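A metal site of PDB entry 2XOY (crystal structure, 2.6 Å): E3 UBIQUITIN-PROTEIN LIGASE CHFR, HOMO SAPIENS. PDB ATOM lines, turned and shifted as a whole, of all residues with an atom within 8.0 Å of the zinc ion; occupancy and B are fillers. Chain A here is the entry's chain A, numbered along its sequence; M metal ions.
SG of Cys 232 lies close to N of Trp 234 (3.4 Å).
SG of Cys 238 lies close to N of Thr 240 (3.3 Å).
The backbone carbonyl oxygen (O) of Cys 232 is in hydrogen-bond range of the side-chain sulfur (SG) of Cys 254, at 3.6 Å.
ND1 of His 252 sits at hydrogen-bond distance from O of Phe 250 (3.2 Å).
The backbone carbonyl oxygen of Cys 238 is in hydrogen-bond range of the side-chain amide nitrogen of Gln 241 (3.2 Å).
The backbone NH (N) of Cys 232 sits at hydrogen-bond distance from the backbone carbonyl oxygen (O) of Asn 251, at 3.0 Å.
Within 4 Å of the zinc ion: Cys 232, Cys 238, His 246 and His 252.
The nearest printed residue that does not touch the zinc ion is Gln 241 (4.5 Å).
The zinc ion is bound by a ring nitrogen (NE2) of His 246, a ring nitrogen (NE2) of His 252, the side-chain sulfur of Cys 238 and the side-chain sulfur of Cys 232.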
ATOM      1  N   ASN A 150     -26.005  -3.536   6.114  1.00  0.00           N
ATOM      2  CA  ASN A 150     -25.625  -3.231   4.750  1.00  0.00           C
ATOM      3  C   ASN A 150     -26.673  -2.285   4.129  1.00  0.00           C
ATOM      4  O   ASN A 150     -27.784  -2.691   3.788  1.00  0.00           O
ATOM      5  CB  ASN A 150     -25.477  -4.536   3.984  1.00  0.00           C
ATOM      6  CG  ASN A 150     -25.149  -4.340   2.530  1.00  0.00           C
ATOM      7  OD1 ASN A 150     -25.535  -3.335   1.918  1.00  0.00           O
ATOM      8  ND2 ASN A 150     -24.439  -5.299   1.947  1.00  0.00           N
ATOM      9  N   PRO A 230     -24.544 -10.704  -9.166  1.00  0.00           N
ATOM     10  CA  PRO A 230     -24.102 -12.071  -8.835  1.00  0.00           C
ATOM     11  C   PRO A 230     -23.936 -12.229  -7.333  1.00  0.00           C
ATOM     12  O   PRO A 230     -23.633 -11.261  -6.627  1.00  0.00           O
ATOM     13  CB  PRO A 230     -22.720 -12.169  -9.475  1.00  0.00           C
ATOM     14  CG  PRO A 230     -22.400 -10.791 -10.055  1.00  0.00           C
ATOM     15  CD  PRO A 230     -23.415  -9.820  -9.512  1.00  0.00           C
ATOM     16  N   ASP A 231     -24.140 -13.444  -6.869  1.00  0.00           N
ATOM     17  CA  ASP A 231     -23.958 -13.748  -5.457  1.00  0.00           C
ATOM     18  C   ASP A 231     -22.507 -13.548  -5.038  1.00  0.00           C
ATOM     19  O   ASP A 231     -21.589 -13.910  -5.767  1.00  0.00           O
ATOM     20  CB  ASP A 231     -24.357 -15.194  -5.186  1.00  0.00           C
ATOM     21  CG  ASP A 231     -25.838 -15.392  -5.153  1.00  0.00           C
ATOM     22  OD1 ASP A 231     -26.567 -14.427  -5.505  1.00  0.00           O
ATOM     23  OD2 ASP A 231     -26.277 -16.483  -4.757  1.00  0.00           O
ATOM     24  N   CYS A 232     -22.293 -12.966  -3.871  1.00  0.00           N
ATOM     25  CA  CYS A 232     -20.949 -12.967  -3.318  1.00  0.00           C
ATOM     26  C   CYS A 232     -20.639 -14.364  -2.842  1.00  0.00           C
ATOM     27  O   CYS A 232     -21.500 -15.020  -2.232  1.00  0.00           O
ATOM     28  CB  CYS A 232     -20.831 -12.016  -2.144  1.00  0.00           C
ATOM     29  SG  CYS A 232     -19.152 -11.960  -1.474  1.00  0.00           S
ATOM     30  N   TYR A 233     -19.421 -14.813  -3.125  1.00  0.00           N
ATOM     31  CA  TYR A 233     -18.912 -16.100  -2.667  1.00  0.00           C
ATOM     32  C   TYR A 233     -19.027 -16.290  -1.149  1.00  0.00           C
ATOM     33  O   TYR A 233     -19.255 -17.403  -0.677  1.00  0.00           O
ATOM     34  CB  TYR A 233     -17.450 -16.253  -3.110  1.00  0.00           C
ATOM     35  CG  TYR A 233     -16.833 -17.597  -2.846  1.00  0.00           C
ATOM     36  CD1 TYR A 233     -16.248 -17.888  -1.602  1.00  0.00           C
ATOM     37  CD2 TYR A 233     -16.805 -18.577  -3.842  1.00  0.00           C
ATOM     38  CE1 TYR A 233     -15.676 -19.128  -1.363  1.00  0.00           C
ATOM     39  CE2 TYR A 233     -16.233 -19.817  -3.603  1.00  0.00           C
ATOM     40  CZ  TYR A 233     -15.672 -20.081  -2.367  1.00  0.00           C
ATOM     41  OH  TYR A 233     -15.107 -21.327  -2.123  1.00  0.00           O
ATOM     42  N   TRP A 234     -18.905 -15.200  -0.402  1.00  0.00           N
ATOM     43  CA  TRP A 234     -18.889 -15.244   1.071  1.00  0.00           C
ATOM     44  C   TRP A 234     -20.271 -15.074   1.702  1.00  0.00           C
ATOM     45  O   TRP A 234     -20.420 -15.232   2.920  1.00  0.00           O
ATOM     46  CB  TRP A 234     -17.917 -14.212   1.651  1.00  0.00           C
ATOM     47  CG  TRP A 234     -16.579 -14.182   0.950  1.00  0.00           C
ATOM     48  CD1 TRP A 234     -16.131 -13.235   0.086  1.00  0.00           C
ATOM     49  CD2 TRP A 234     -15.525 -15.145   1.064  1.00  0.00           C
ATOM     50  NE1 TRP A 234     -14.880 -13.550  -0.369  1.00  0.00           N
ATOM     51  CE2 TRP A 234     -14.477 -14.715   0.225  1.00  0.00           C
ATOM     52  CE3 TRP A 234     -15.370 -16.329   1.784  1.00  0.00           C
ATOM     53  CZ2 TRP A 234     -13.293 -15.422   0.108  1.00  0.00           C
ATOM     54  CZ3 TRP A 234     -14.191 -17.035   1.659  1.00  0.00           C
ATOM     55  CH2 TRP A 234     -13.167 -16.576   0.836  1.00  0.00           C
ATOM     56  N   GLY A 235     -21.264 -14.750   0.885  1.00  0.00           N
ATOM     57  CA  GLY A 235     -22.638 -14.696   1.361  1.00  0.00           C
ATOM     58  C   GLY A 235     -22.965 -13.623   2.392  1.00  0.00           C
ATOM     59  O   GLY A 235     -22.346 -12.568   2.438  1.00  0.00           O
ATOM     60  N   ARG A 236     -23.959 -13.907   3.214  1.00  0.00           N
ATOM     61  CA  ARG A 236     -24.538 -12.894   4.084  1.00  0.00           C
ATOM     62  C   ARG A 236     -23.539 -12.388   5.114  1.00  0.00           C
ATOM     63  O   ARG A 236     -23.702 -11.308   5.677  1.00  0.00           O
ATOM     64  CB  ARG A 236     -25.747 -13.496   4.806  1.00  0.00           C
ATOM     65  CG  ARG A 236     -25.397 -14.787   5.525  1.00  0.00           C
ATOM     66  CD  ARG A 236     -26.612 -15.536   5.969  1.00  0.00           C
ATOM     67  NE  ARG A 236     -27.381 -14.760   6.930  1.00  0.00           N
ATOM     68  CZ  ARG A 236     -28.488 -15.203   7.532  1.00  0.00           C
ATOM     69  NH1 ARG A 236     -28.942 -16.427   7.262  1.00  0.00           N
ATOM     70  NH2 ARG A 236     -29.141 -14.429   8.392  1.00  0.00           N
ATOM     71  N   ASN A 237     -22.488 -13.166   5.358  1.00  0.00           N
ATOM     72  CA  ASN A 237     -21.582 -12.837   6.441  1.00  0.00           C
ATOM     73  C   ASN A 237     -20.310 -12.177   5.968  1.00  0.00           C
ATOM     74  O   ASN A 237     -19.491 -11.742   6.765  1.00  0.00           O
ATOM     75  CB  ASN A 237     -21.305 -14.052   7.343  1.00  0.00           C
ATOM     76  CG  ASN A 237     -22.472 -14.372   8.242  1.00  0.00           C
ATOM     77  OD1 ASN A 237     -23.003 -13.494   8.931  1.00  0.00           O
ATOM     78  ND2 ASN A 237     -22.898 -15.630   8.239  1.00  0.00           N
ATOM     79  N   CYS A 238     -20.196 -12.059   4.651  1.00  0.00           N
ATOM     80  CA  CYS A 238     -19.104 -11.328   4.035  1.00  0.00           C
ATOM     81  C   CYS A 238     -18.696 -10.084   4.817  1.00  0.00           C
ATOM     82  O   CYS A 238     -19.537  -9.299   5.262  1.00  0.00           O
ATOM     83  CB  CYS A 238     -19.504 -10.941   2.626  1.00  0.00           C
ATOM     84  SG  CYS A 238     -18.301  -9.964   1.781  1.00  0.00           S
ATOM     85  N   ARG A 239     -17.391  -9.891   4.996  1.00  0.00           N
ATOM     86  CA  ARG A 239     -16.879  -8.736   5.740  1.00  0.00           C
ATOM     87  C   ARG A 239     -16.682  -7.503   4.851  1.00  0.00           C
ATOM     88  O   ARG A 239     -16.633  -6.394   5.347  1.00  0.00           O
ATOM     89  CB  ARG A 239     -15.564  -9.078   6.441  1.00  0.00           C
ATOM     90  CG  ARG A 239     -15.656 -10.229   7.433  1.00  0.00           C
ATOM     91  CD  ARG A 239     -16.371  -9.811   8.702  1.00  0.00           C
ATOM     92  NE  ARG A 239     -15.744 -10.380   9.905  1.00  0.00           N
ATOM     93  CZ  ARG A 239     -16.165 -11.478  10.541  1.00  0.00           C
ATOM     94  NH1 ARG A 239     -15.507 -11.916  11.610  1.00  0.00           N
ATOM     95  NH2 ARG A 239     -17.245 -12.144  10.097  1.00  0.00           N
ATOM     96  N   THR A 240     -16.590  -7.722   3.546  1.00  0.00           N
ATOM     97  CA  THR A 240     -16.329  -6.653   2.582  1.00  0.00           C
ATOM     98  C   THR A 240     -17.583  -5.877   2.208  1.00  0.00           C
ATOM     99  O   THR A 240     -17.513  -4.837   1.537  1.00  0.00           O
ATOM    100  CB  THR A 240     -15.733  -7.221   1.289  1.00  0.00           C
ATOM    101  OG1 THR A 240     -14.664  -8.111   1.612  1.00  0.00           O
ATOM    102  CG2 THR A 240     -15.213  -6.104   0.397  1.00  0.00           C
ATOM    103  N   GLN A 241     -18.737  -6.384   2.599  1.00  0.00           N
ATOM    104  CA  GLN A 241     -19.997  -5.766   2.175  1.00  0.00           C
ATOM    105  C   GLN A 241     -20.302  -4.419   2.843  1.00  0.00           C
ATOM    106  O   GLN A 241     -21.282  -3.758   2.500  1.00  0.00           O
ATOM    107  CB  GLN A 241     -21.163  -6.738   2.325  1.00  0.00           C
ATOM    108  CG  GLN A 241     -21.571  -7.001   3.733  1.00  0.00           C
ATOM    109  CD  GLN A 241     -22.738  -7.937   3.813  1.00  0.00           C
ATOM    110  OE1 GLN A 241     -23.756  -7.714   3.151  1.00  0.00           O
ATOM    111  NE2 GLN A 241     -22.606  -8.984   4.603  1.00  0.00           N
ATOM    112  N   VAL A 242     -19.453  -3.983   3.777  1.00  0.00           N
ATOM    113  CA  VAL A 242     -19.640  -2.673   4.378  1.00  0.00           C
ATOM    114  C   VAL A 242     -18.911  -1.580   3.598  1.00  0.00           C
ATOM    115  O   VAL A 242     -18.857  -0.436   4.033  1.00  0.00           O
ATOM    116  CB  VAL A 242     -19.199  -2.629   5.863  1.00  0.00           C
ATOM    117  CG1 VAL A 242     -20.051  -3.602   6.729  1.00  0.00           C
ATOM    118  CG2 VAL A 242     -17.697  -2.908   5.999  1.00  0.00           C
ATOM    119  N   HIS A 246     -18.541  -2.674  -3.178  1.00  0.00           N
ATOM    120  CA  HIS A 246     -18.763  -4.126  -3.084  1.00  0.00           C
ATOM    121  C   HIS A 246     -20.220  -4.491  -2.739  1.00  0.00           C
ATOM    122  O   HIS A 246     -20.770  -5.426  -3.305  1.00  0.00           O
ATOM    123  CB  HIS A 246     -17.812  -4.734  -2.036  1.00  0.00           C
ATOM    124  CG  HIS A 246     -17.918  -6.216  -1.900  1.00  0.00           C
ATOM    125  ND1 HIS A 246     -17.330  -7.093  -2.782  1.00  0.00           N
ATOM    126  CD2 HIS A 246     -18.540  -6.989  -0.973  1.00  0.00           C
ATOM    127  CE1 HIS A 246     -17.590  -8.335  -2.414  1.00  0.00           C
ATOM    128  NE2 HIS A 246     -18.321  -8.292  -1.319  1.00  0.00           N
ATOM    129  N   ALA A 247     -20.828  -3.765  -1.815  1.00  0.00           N
ATOM    130  CA  ALA A 247     -22.229  -3.998  -1.477  1.00  0.00           C
ATOM    131  C   ALA A 247     -23.097  -3.873  -2.721  1.00  0.00           C
ATOM    132  O   ALA A 247     -24.000  -4.680  -2.928  1.00  0.00           O
ATOM    133  CB  ALA A 247     -22.722  -3.041  -0.402  1.00  0.00           C
ATOM    134  N   LYS A 249     -22.161  -4.169  -5.868  1.00  0.00           N
ATOM    135  CA  LYS A 249     -21.763  -5.033  -6.972  1.00  0.00           C
ATOM    136  C   LYS A 249     -22.258  -6.475  -6.805  1.00  0.00           C
ATOM    137  O   LYS A 249     -22.571  -7.138  -7.803  1.00  0.00           O
ATOM    138  CB  LYS A 249     -20.249  -5.002  -7.177  1.00  0.00           C
ATOM    139  CG  LYS A 249     -19.772  -5.955  -8.253  1.00  0.00           C
ATOM    140  CD  LYS A 249     -18.275  -5.804  -8.526  1.00  0.00           C
ATOM    141  CE  LYS A 249     -17.790  -6.794  -9.585  1.00  0.00           C
ATOM    142  NZ  LYS A 249     -16.446  -6.416 -10.118  1.00  0.00           N
ATOM    143  N   PHE A 250     -22.341  -6.947  -5.561  1.00  0.00           N
ATOM    144  CA  PHE A 250     -22.748  -8.325  -5.294  1.00  0.00           C
ATOM    145  C   PHE A 250     -23.992  -8.456  -4.444  1.00  0.00           C
ATOM    146  O   PHE A 250     -24.266  -7.636  -3.580  1.00  0.00           O
ATOM    147  CB  PHE A 250     -21.641  -9.139  -4.610  1.00  0.00           C
ATOM    148  CG  PHE A 250     -20.387  -9.253  -5.406  1.00  0.00           C
ATOM    149  CD1 PHE A 250     -19.363  -8.327  -5.248  1.00  0.00           C
ATOM    150  CD2 PHE A 250     -20.214 -10.299  -6.285  1.00  0.00           C
ATOM    151  CE1 PHE A 250     -18.195  -8.440  -5.963  1.00  0.00           C
ATOM    152  CE2 PHE A 250     -19.038 -10.429  -7.006  1.00  0.00           C
ATOM    153  CZ  PHE A 250     -18.039  -9.505  -6.845  1.00  0.00           C
ATOM    154  N   ASN A 251     -24.724  -9.543  -4.681  1.00  0.00           N
ATOM    155  CA  ASN A 251     -25.859  -9.894  -3.853  1.00  0.00           C
ATOM    156  C   ASN A 251     -25.368 -10.600  -2.602  1.00  0.00           C
ATOM    157  O   ASN A 251     -24.666 -11.601  -2.677  1.00  0.00           O
ATOM    158  CB  ASN A 251     -26.847 -10.783  -4.631  1.00  0.00           C
ATOM    159  CG  ASN A 251     -27.870 -11.445  -3.722  1.00  0.00           C
ATOM    160  OD1 ASN A 251     -28.559 -10.784  -2.952  1.00  0.00           O
ATOM    161  ND2 ASN A 251     -27.953 -12.766  -3.787  1.00  0.00           N
ATOM    162  N   HIS A 252     -25.756 -10.076  -1.436  1.00  0.00           N
ATOM    163  CA  HIS A 252     -25.417 -10.668  -0.151  1.00  0.00           C
ATOM    164  C   HIS A 252     -26.622 -11.226   0.582  1.00  0.00           C
ATOM    165  O   HIS A 252     -26.550 -11.484   1.782  1.00  0.00           O
ATOM    166  CB  HIS A 252     -24.686  -9.667   0.729  1.00  0.00           C
ATOM    167  CG  HIS A 252     -23.344  -9.294   0.209  1.00  0.00           C
ATOM    168  ND1 HIS A 252     -23.140  -8.184  -0.583  1.00  0.00           N
ATOM    169  CD2 HIS A 252     -22.139  -9.895   0.347  1.00  0.00           C
ATOM    170  CE1 HIS A 252     -21.863  -8.125  -0.919  1.00  0.00           C
ATOM    171  NE2 HIS A 252     -21.241  -9.151  -0.367  1.00  0.00           N
ATOM    172  N   CYS A 254     -27.599 -14.263   0.444  1.00  0.00           N
ATOM    173  CA  CYS A 254     -27.270 -15.632   0.071  1.00  0.00           C
ATOM    174  C   CYS A 254     -26.395 -16.280   1.131  1.00  0.00           C
ATOM    175  O   CYS A 254     -25.895 -15.620   2.053  1.00  0.00           O
ATOM    176  CB  CYS A 254     -26.582 -15.704  -1.297  1.00  0.00           C
ATOM    177  SG  CYS A 254     -25.058 -14.756  -1.469  1.00  0.00           S
HETATM  178 ZN    ZN M   1     -19.176  -9.847  -0.309  1.00  0.00          ZN
